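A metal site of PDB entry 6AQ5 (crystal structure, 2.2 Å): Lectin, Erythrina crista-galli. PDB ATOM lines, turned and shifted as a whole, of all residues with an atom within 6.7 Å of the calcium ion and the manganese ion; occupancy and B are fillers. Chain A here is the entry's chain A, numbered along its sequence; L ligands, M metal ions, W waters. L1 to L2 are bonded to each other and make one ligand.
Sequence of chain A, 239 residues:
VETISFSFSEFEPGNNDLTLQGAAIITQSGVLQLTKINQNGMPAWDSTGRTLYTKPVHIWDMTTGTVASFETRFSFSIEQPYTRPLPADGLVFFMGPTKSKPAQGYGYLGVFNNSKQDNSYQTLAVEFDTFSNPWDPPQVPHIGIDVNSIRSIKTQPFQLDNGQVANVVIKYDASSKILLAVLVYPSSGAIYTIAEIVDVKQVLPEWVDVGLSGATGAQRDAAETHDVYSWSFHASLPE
The side-chain amide oxygen (OD1) of Asn 133 is in hydrogen-bond range of an oxygen (O2) of LG2 L2 (2.9 Å).
The backbone NH (N) of Gly 107 sits at hydrogen-bond distance from an oxygen (O2) of LG2 L2, 3.1 Å away.
OD1 of Asp 89 lies within hydrogen-bond range of O3 of LG2 L2, 2.6 Å away.
The side-chain carboxylate of Glu 127 lies close to the side-chain carboxylate of Asp 146.
N of Glu 127 lies within hydrogen-bond range of O of Gly 144, 2.8 Å away.
Of the 23 residues printed, 4 come within 4 Å of the manganese ion.
The calcium ion is bound by ND2 of Asn 133 (2.3 Å), OD2 of Asp 136 (2.3 Å), O of Phe 131 (2.3 Å), water W4 (2.4 Å), OD2 of Asp 129 (2.4 Å), water W2 (2.4 Å) and OD1 of Asp 129 (2.5 Å).
The manganese ion is bound by the side-chain carboxylate (OE2) of Glu 127, the side-chain carboxylate (OD1) of Asp 136, water W1, the side-chain carboxylate (OD2) of Asp 129, a ring nitrogen (NE2) of His 142 and water W3.
Water W2 lies within hydrogen-bond range of O of Gly 107 and NE1 of Trp 135.
Water W3 lies within hydrogen-bond range of the side-chain carboxylate of Glu 127 and the backbone carbonyl oxygen of Ile 150.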
ATOM      1  N   ASP A  89     -11.666 -26.067   7.730  1.00  0.00           N
ATOM      2  CA  ASP A  89     -11.378 -25.966   9.161  1.00  0.00           C
ATOM      3  C   ASP A  89     -12.080 -24.760   9.809  1.00  0.00           C
ATOM      4  O   ASP A  89     -12.322 -24.767  11.015  1.00  0.00           O
ATOM      5  CB  ASP A  89      -9.869 -25.859   9.401  1.00  0.00           C
ATOM      6  CG  ASP A  89      -9.206 -27.218   9.607  1.00  0.00           C
ATOM      7  OD1 ASP A  89      -8.612 -27.736   8.640  1.00  0.00           O
ATOM      8  OD2 ASP A  89      -9.288 -27.754  10.725  1.00  0.00           O
ATOM      9  N   TYR A 106      -4.946 -25.334   8.125  1.00  0.00           N
ATOM     10  CA  TYR A 106      -5.729 -26.371   8.819  1.00  0.00           C
ATOM     11  C   TYR A 106      -6.334 -25.736  10.078  1.00  0.00           C
ATOM     12  O   TYR A 106      -6.817 -24.603  10.005  1.00  0.00           O
ATOM     13  CB  TYR A 106      -4.852 -27.613   9.061  1.00  0.00           C
ATOM     14  CG  TYR A 106      -4.103 -28.098   7.840  1.00  0.00           C
ATOM     15  CD1 TYR A 106      -2.831 -28.678   7.961  1.00  0.00           C
ATOM     16  CD2 TYR A 106      -4.646 -28.005   6.561  1.00  0.00           C
ATOM     17  CE1 TYR A 106      -2.122 -29.122   6.835  1.00  0.00           C
ATOM     18  CE2 TYR A 106      -3.945 -28.455   5.433  1.00  0.00           C
ATOM     19  CZ  TYR A 106      -2.686 -29.012   5.574  1.00  0.00           C
ATOM     20  OH  TYR A 106      -1.993 -29.466   4.481  1.00  0.00           O
ATOM     21  N   GLY A 107      -6.299 -26.414  11.235  1.00  0.00           N
ATOM     22  CA  GLY A 107      -6.948 -25.909  12.429  1.00  0.00           C
ATOM     23  C   GLY A 107      -6.286 -24.693  13.036  1.00  0.00           C
ATOM     24  O   GLY A 107      -6.824 -24.145  14.004  1.00  0.00           O
ATOM     25  N   TYR A 108      -5.154 -24.274  12.501  1.00  0.00           N
ATOM     26  CA  TYR A 108      -4.560 -23.004  12.909  1.00  0.00           C
ATOM     27  C   TYR A 108      -5.102 -21.829  12.102  1.00  0.00           C
ATOM     28  O   TYR A 108      -4.718 -20.682  12.362  1.00  0.00           O
ATOM     29  CB  TYR A 108      -3.024 -23.083  12.781  1.00  0.00           C
ATOM     30  CG  TYR A 108      -2.458 -24.332  13.429  1.00  0.00           C
ATOM     31  CD1 TYR A 108      -2.502 -24.517  14.799  1.00  0.00           C
ATOM     32  CD2 TYR A 108      -1.905 -25.351  12.648  1.00  0.00           C
ATOM     33  CE1 TYR A 108      -2.015 -25.663  15.387  1.00  0.00           C
ATOM     34  CE2 TYR A 108      -1.412 -26.499  13.227  1.00  0.00           C
ATOM     35  CZ  TYR A 108      -1.468 -26.657  14.603  1.00  0.00           C
ATOM     36  OH  TYR A 108      -0.967 -27.800  15.186  1.00  0.00           O
ATOM     37  N   LEU A 109      -5.983 -22.096  11.141  1.00  0.00           N
ATOM     38  CA  LEU A 109      -6.830 -21.105  10.483  1.00  0.00           C
ATOM     39  C   LEU A 109      -6.019 -20.006   9.795  1.00  0.00           C
ATOM     40  O   LEU A 109      -6.571 -18.955   9.461  1.00  0.00           O
ATOM     41  CB  LEU A 109      -7.826 -20.503  11.480  1.00  0.00           C
ATOM     42  CG  LEU A 109      -8.746 -21.515  12.159  1.00  0.00           C
ATOM     43  CD1 LEU A 109      -9.699 -20.841  13.130  1.00  0.00           C
ATOM     44  CD2 LEU A 109      -9.542 -22.324  11.127  1.00  0.00           C
ATOM     45  N   GLU A 127     -13.006 -16.643  16.249  1.00  0.00           N
ATOM     46  CA  GLU A 127     -12.984 -17.717  15.272  1.00  0.00           C
ATOM     47  C   GLU A 127     -14.372 -18.322  15.096  1.00  0.00           C
ATOM     48  O   GLU A 127     -15.191 -18.320  16.008  1.00  0.00           O
ATOM     49  CB  GLU A 127     -11.999 -18.815  15.671  1.00  0.00           C
ATOM     50  CG  GLU A 127     -12.372 -19.526  16.956  1.00  0.00           C
ATOM     51  CD  GLU A 127     -11.558 -20.779  17.210  1.00  0.00           C
ATOM     52  OE1 GLU A 127     -10.325 -20.745  17.028  1.00  0.00           O
ATOM     53  OE2 GLU A 127     -12.148 -21.811  17.573  1.00  0.00           O
ATOM     54  N   ASP A 129     -15.202 -21.909  13.971  1.00  0.00           N
ATOM     55  CA  ASP A 129     -14.376 -23.108  13.834  1.00  0.00           C
ATOM     56  C   ASP A 129     -15.280 -24.293  13.496  1.00  0.00           C
ATOM     57  O   ASP A 129     -16.221 -24.588  14.229  1.00  0.00           O
ATOM     58  CB  ASP A 129     -13.607 -23.338  15.137  1.00  0.00           C
ATOM     59  CG  ASP A 129     -12.602 -24.461  15.042  1.00  0.00           C
ATOM     60  OD1 ASP A 129     -12.585 -25.210  14.039  1.00  0.00           O
ATOM     61  OD2 ASP A 129     -11.801 -24.601  16.004  1.00  0.00           O
ATOM     62  N   THR A 130     -14.965 -24.987  12.395  1.00  0.00           N
ATOM     63  CA  THR A 130     -15.815 -26.058  11.904  1.00  0.00           C
ATOM     64  C   THR A 130     -15.265 -27.461  12.114  1.00  0.00           C
ATOM     65  O   THR A 130     -15.972 -28.431  11.823  1.00  0.00           O
ATOM     66  CB  THR A 130     -16.093 -25.849  10.400  1.00  0.00           C
ATOM     67  OG1 THR A 130     -14.855 -25.715   9.700  1.00  0.00           O
ATOM     68  CG2 THR A 130     -16.925 -24.591  10.183  1.00  0.00           C
ATOM     69  N   PHE A 131     -14.033 -27.600  12.615  1.00  0.00           N
ATOM     70  CA  PHE A 131     -13.447 -28.909  12.849  1.00  0.00           C
ATOM     71  C   PHE A 131     -12.890 -28.996  14.264  1.00  0.00           C
ATOM     72  O   PHE A 131     -12.181 -28.088  14.700  1.00  0.00           O
ATOM     73  CB  PHE A 131     -12.338 -29.216  11.830  1.00  0.00           C
ATOM     74  CG  PHE A 131     -11.716 -30.578  12.009  1.00  0.00           C
ATOM     75  CD1 PHE A 131     -12.208 -31.677  11.328  1.00  0.00           C
ATOM     76  CD2 PHE A 131     -10.647 -30.759  12.879  1.00  0.00           C
ATOM     77  CE1 PHE A 131     -11.648 -32.932  11.508  1.00  0.00           C
ATOM     78  CE2 PHE A 131     -10.076 -32.015  13.067  1.00  0.00           C
ATOM     79  CZ  PHE A 131     -10.576 -33.100  12.375  1.00  0.00           C
ATOM     80  N   SER A 132     -13.203 -30.082  14.961  1.00  0.00           N
ATOM     81  CA  SER A 132     -12.790 -30.247  16.359  1.00  0.00           C
ATOM     82  C   SER A 132     -11.386 -30.837  16.396  1.00  0.00           C
ATOM     83  O   SER A 132     -11.204 -32.058  16.269  1.00  0.00           O
ATOM     84  CB  SER A 132     -13.782 -31.108  17.117  1.00  0.00           C
ATOM     85  OG  SER A 132     -13.469 -31.130  18.501  1.00  0.00           O
ATOM     86  N   ASN A 133     -10.392 -29.980  16.562  1.00  0.00           N
ATOM     87  CA  ASN A 133      -9.007 -30.385  16.753  1.00  0.00           C
ATOM     88  C   ASN A 133      -8.806 -30.835  18.202  1.00  0.00           C
ATOM     89  O   ASN A 133      -9.680 -30.640  19.045  1.00  0.00           O
ATOM     90  CB  ASN A 133      -8.085 -29.221  16.399  1.00  0.00           C
ATOM     91  CG  ASN A 133      -8.078 -28.895  14.917  1.00  0.00           C
ATOM     92  OD1 ASN A 133      -7.346 -29.516  14.144  1.00  0.00           O
ATOM     93  ND2 ASN A 133      -8.872 -27.915  14.522  1.00  0.00           N
ATOM     94  N   TRP A 135      -7.241 -29.581  20.558  1.00  0.00           N
ATOM     95  CA  TRP A 135      -7.305 -28.449  21.480  1.00  0.00           C
ATOM     96  C   TRP A 135      -8.682 -27.784  21.534  1.00  0.00           C
ATOM     97  O   TRP A 135      -8.841 -26.780  22.224  1.00  0.00           O
ATOM     98  CB  TRP A 135      -6.258 -27.403  21.084  1.00  0.00           C
ATOM     99  CG  TRP A 135      -6.330 -27.011  19.635  1.00  0.00           C
ATOM    100  CD1 TRP A 135      -7.160 -26.082  19.079  1.00  0.00           C
ATOM    101  CD2 TRP A 135      -5.543 -27.538  18.561  1.00  0.00           C
ATOM    102  NE1 TRP A 135      -6.945 -25.997  17.730  1.00  0.00           N
ATOM    103  CE2 TRP A 135      -5.957 -26.878  17.377  1.00  0.00           C
ATOM    104  CE3 TRP A 135      -4.534 -28.505  18.467  1.00  0.00           C
ATOM    105  CZ2 TRP A 135      -5.390 -27.148  16.130  1.00  0.00           C
ATOM    106  CZ3 TRP A 135      -3.973 -28.771  17.228  1.00  0.00           C
ATOM    107  CH2 TRP A 135      -4.405 -28.105  16.081  1.00  0.00           C
ATOM    108  N   ASP A 136      -9.679 -28.323  20.815  1.00  0.00           N
ATOM    109  CA  ASP A 136     -11.005 -27.749  20.672  1.00  0.00           C
ATOM    110  C   ASP A 136     -11.993 -28.401  21.615  1.00  0.00           C
ATOM    111  O   ASP A 136     -11.775 -29.521  22.105  1.00  0.00           O
ATOM    112  CB  ASP A 136     -11.509 -27.945  19.234  1.00  0.00           C
ATOM    113  CG  ASP A 136     -10.950 -26.918  18.281  1.00  0.00           C
ATOM    114  OD1 ASP A 136     -10.811 -25.751  18.697  1.00  0.00           O
ATOM    115  OD2 ASP A 136     -10.661 -27.280  17.124  1.00  0.00           O
ATOM    116  N   PRO A 137     -13.112 -27.741  21.905  1.00  0.00           N
ATOM    117  CA  PRO A 137     -14.259 -28.448  22.474  1.00  0.00           C
ATOM    118  C   PRO A 137     -14.786 -29.476  21.492  1.00  0.00           C
ATOM    119  O   PRO A 137     -14.441 -29.418  20.298  1.00  0.00           O
ATOM    120  CB  PRO A 137     -15.277 -27.328  22.729  1.00  0.00           C
ATOM    121  CG  PRO A 137     -14.905 -26.263  21.758  1.00  0.00           C
ATOM    122  CD  PRO A 137     -13.411 -26.317  21.655  1.00  0.00           C
ATOM    123  N   VAL A 140     -18.722 -28.845  17.034  1.00  0.00           N
ATOM    124  CA  VAL A 140     -18.457 -27.945  15.916  1.00  0.00           C
ATOM    125  C   VAL A 140     -19.754 -27.782  15.126  1.00  0.00           C
ATOM    126  O   VAL A 140     -20.573 -28.703  15.073  1.00  0.00           O
ATOM    127  CB  VAL A 140     -17.323 -28.462  15.018  1.00  0.00           C
ATOM    128  CG1 VAL A 140     -15.983 -28.221  15.691  1.00  0.00           C
ATOM    129  CG2 VAL A 140     -17.509 -29.938  14.702  1.00  0.00           C
ATOM    130  N   HIS A 142     -18.233 -23.890  16.284  1.00  0.00           N
ATOM    131  CA  HIS A 142     -18.300 -23.091  17.503  1.00  0.00           C
ATOM    132  C   HIS A 142     -17.649 -21.756  17.248  1.00  0.00           C
ATOM    133  O   HIS A 142     -16.714 -21.634  16.443  1.00  0.00           O
ATOM    134  CB  HIS A 142     -17.636 -23.799  18.701  1.00  0.00           C
ATOM    135  CG  HIS A 142     -16.198 -24.159  18.482  1.00  0.00           C
ATOM    136  ND1 HIS A 142     -15.777 -25.441  18.239  1.00  0.00           N
ATOM    137  CD2 HIS A 142     -15.077 -23.389  18.490  1.00  0.00           C
ATOM    138  CE1 HIS A 142     -14.459 -25.464  18.102  1.00  0.00           C
ATOM    139  NE2 HIS A 142     -14.016 -24.225  18.247  1.00  0.00           N
ATOM    140  N   ILE A 143     -18.183 -20.726  17.909  1.00  0.00           N
ATOM    141  CA  ILE A 143     -17.494 -19.442  18.014  1.00  0.00           C
ATOM    142  C   ILE A 143     -16.439 -19.548  19.089  1.00  0.00           C
ATOM    143  O   ILE A 143     -16.646 -20.216  20.110  1.00  0.00           O
ATOM    144  CB  ILE A 143     -18.483 -18.316  18.326  1.00  0.00           C
ATOM    145  CG1 ILE A 143     -19.772 -18.452  17.488  1.00  0.00           C
ATOM    146  CG2 ILE A 143     -17.838 -16.951  18.093  1.00  0.00           C
ATOM    147  CD1 ILE A 143     -20.874 -17.494  17.909  1.00  0.00           C
ATOM    148  N   GLY A 144     -15.304 -18.899  18.886  1.00  0.00           N
ATOM    149  CA  GLY A 144     -14.282 -18.890  19.900  1.00  0.00           C
ATOM    150  C   GLY A 144     -13.588 -17.563  20.003  1.00  0.00           C
ATOM    151  O   GLY A 144     -13.328 -16.897  18.995  1.00  0.00           O
ATOM    152  N   ASP A 146     -10.159 -16.082  20.803  1.00  0.00           N
ATOM    153  CA  ASP A 146      -8.777 -16.532  20.803  1.00  0.00           C
ATOM    154  C   ASP A 146      -7.869 -15.382  21.250  1.00  0.00           C
ATOM    155  O   ASP A 146      -7.798 -14.354  20.575  1.00  0.00           O
ATOM    156  CB  ASP A 146      -8.344 -17.023  19.426  1.00  0.00           C
ATOM    157  CG  ASP A 146      -9.168 -18.196  18.945  1.00  0.00           C
ATOM    158  OD1 ASP A 146      -9.947 -18.760  19.738  1.00  0.00           O
ATOM    159  OD2 ASP A 146      -9.032 -18.535  17.747  1.00  0.00           O
ATOM    160  N   ILE A 150      -4.630 -20.537  19.478  1.00  0.00           N
ATOM    161  CA  ILE A 150      -5.750 -21.154  18.797  1.00  0.00           C
ATOM    162  C   ILE A 150      -6.667 -21.850  19.795  1.00  0.00           C
ATOM    163  O   ILE A 150      -7.841 -22.106  19.491  1.00  0.00           O
ATOM    164  CB  ILE A 150      -5.261 -22.125  17.703  1.00  0.00           C
ATOM    165  CG1 ILE A 150      -6.415 -22.540  16.794  1.00  0.00           C
ATOM    166  CG2 ILE A 150      -4.616 -23.348  18.330  1.00  0.00           C
ATOM    167  CD1 ILE A 150      -7.024 -21.415  15.987  1.00  0.00           C
ATOM    168  N   ARG A 151      -6.170 -22.161  20.991  1.00  0.00           N
ATOM    169  CA  ARG A 151      -6.966 -22.742  22.066  1.00  0.00           C
ATOM    170  C   ARG A 151      -7.747 -21.609  22.728  1.00  0.00           C
ATOM    171  O   ARG A 151      -7.199 -20.832  23.509  1.00  0.00           O
ATOM    172  CB  ARG A 151      -6.072 -23.468  23.071  1.00  0.00           C
ATOM    173  CG  ARG A 151      -6.842 -24.202  24.164  1.00  0.00           C
ATOM    174  CD  ARG A 151      -5.900 -24.799  25.226  1.00  0.00           C
ATOM    175  NE  ARG A 151      -4.947 -25.738  24.653  1.00  0.00           N
ATOM    176  CZ  ARG A 151      -5.125 -27.046  24.608  1.00  0.00           C
ATOM    177  NH1 ARG A 151      -6.229 -27.595  25.101  1.00  0.00           N
ATOM    178  NH2 ARG A 151      -4.194 -27.829  24.069  1.00  0.00           N
ATOM    179  N   SER A 152      -9.041 -21.521  22.413  1.00  0.00           N
ATOM    180  CA  SER A 152      -9.845 -20.378  22.810  1.00  0.00           C
ATOM    181  C   SER A 152      -9.983 -20.301  24.325  1.00  0.00           C
ATOM    182  O   SER A 152     -10.082 -21.318  25.015  1.00  0.00           O
ATOM    183  CB  SER A 152     -11.244 -20.471  22.187  1.00  0.00           C
ATOM    184  OG  SER A 152     -11.171 -20.735  20.796  1.00  0.00           O
ATOM    185  N   THR A 155     -15.508 -20.619  24.260  1.00  0.00           N
ATOM    186  CA  THR A 155     -16.151 -21.115  23.046  1.00  0.00           C
ATOM    187  C   THR A 155     -17.648 -21.175  23.235  1.00  0.00           C
ATOM    188  O   THR A 155     -18.152 -21.334  24.360  1.00  0.00           O
ATOM    189  CB  THR A 155     -15.637 -22.506  22.642  1.00  0.00           C
ATOM    190  OG1 THR A 155     -15.907 -23.436  23.692  1.00  0.00           O
ATOM    191  CG2 THR A 155     -14.143 -22.468  22.358  1.00  0.00           C
HETATM  192  C1  LIG L   1      -3.186 -36.812   9.166  1.00  0.00           C
HETATM  193  C2  LIG L   1      -4.355 -36.561   8.261  1.00  0.00           C
HETATM  194  C3  LIG L   1      -4.816 -35.125   8.410  1.00  0.00           C
HETATM  195  C4  LIG L   1      -4.955 -34.731   9.868  1.00  0.00           C
HETATM  196  C5  LIG L   1      -3.871 -35.315  10.765  1.00  0.00           C
HETATM  197  C6  LIG L   1      -4.308 -35.204  12.211  1.00  0.00           C
HETATM  198  O1  LIG L   1      -2.732 -38.121   8.971  1.00  0.00           O
HETATM  199  O2  LIG L   1      -5.412 -37.417   8.620  1.00  0.00           O
HETATM  200  O3  LIG L   1      -6.057 -34.995   7.765  1.00  0.00           O
HETATM  201  O4  LIG L   1      -4.944 -33.328   9.936  1.00  0.00           O
HETATM  202  O5  LIG L   1      -3.630 -36.676  10.493  1.00  0.00           O
HETATM  203  O6  LIG L   1      -3.191 -35.038  13.045  1.00  0.00           O
HETATM  204  C1  LG2 L   2      -6.168 -32.774  10.353  1.00  0.00           C
HETATM  205  C2  LG2 L   2      -6.005 -31.296  10.653  1.00  0.00           C
HETATM  206  C3  LG2 L   2      -7.348 -30.722  11.055  1.00  0.00           C
HETATM  207  C4  LG2 L   2      -8.347 -30.963   9.947  1.00  0.00           C
HETATM  208  C5  LG2 L   2      -8.419 -32.437   9.607  1.00  0.00           C
HETATM  209  C6  LG2 L   2      -9.269 -32.606   8.367  1.00  0.00           C
HETATM  210  O1  LG2 L   2      -5.093 -31.105  11.707  1.00  0.00           O
HETATM  211  O2  LG2 L   2      -7.224 -29.336  11.302  1.00  0.00           O
HETATM  212  O3  LG2 L   2      -7.963 -30.254   8.788  1.00  0.00           O
HETATM  213  O4  LG2 L   2      -7.124 -32.944   9.337  1.00  0.00           O
HETATM  214  O5  LG2 L   2      -9.516 -33.979   8.132  1.00  0.00           O
HETATM  215 CA    CA M   1     -10.571 -26.415  14.977  1.00  0.00          CA
HETATM  216 MN    MN M   2     -11.719 -23.850  18.099  1.00  0.00          MN
HETATM  217  O   HOH W   1     -11.663 -23.039  20.164  1.00  0.00           O
HETATM  218  O   HOH W   2      -8.680 -24.965  15.444  1.00  0.00           O
HETATM  219  O   HOH W   3      -9.558 -23.053  17.649  1.00  0.00           O
HETATM  220  O   HOH W   4     -10.272 -26.172  12.595  1.00  0.00           O
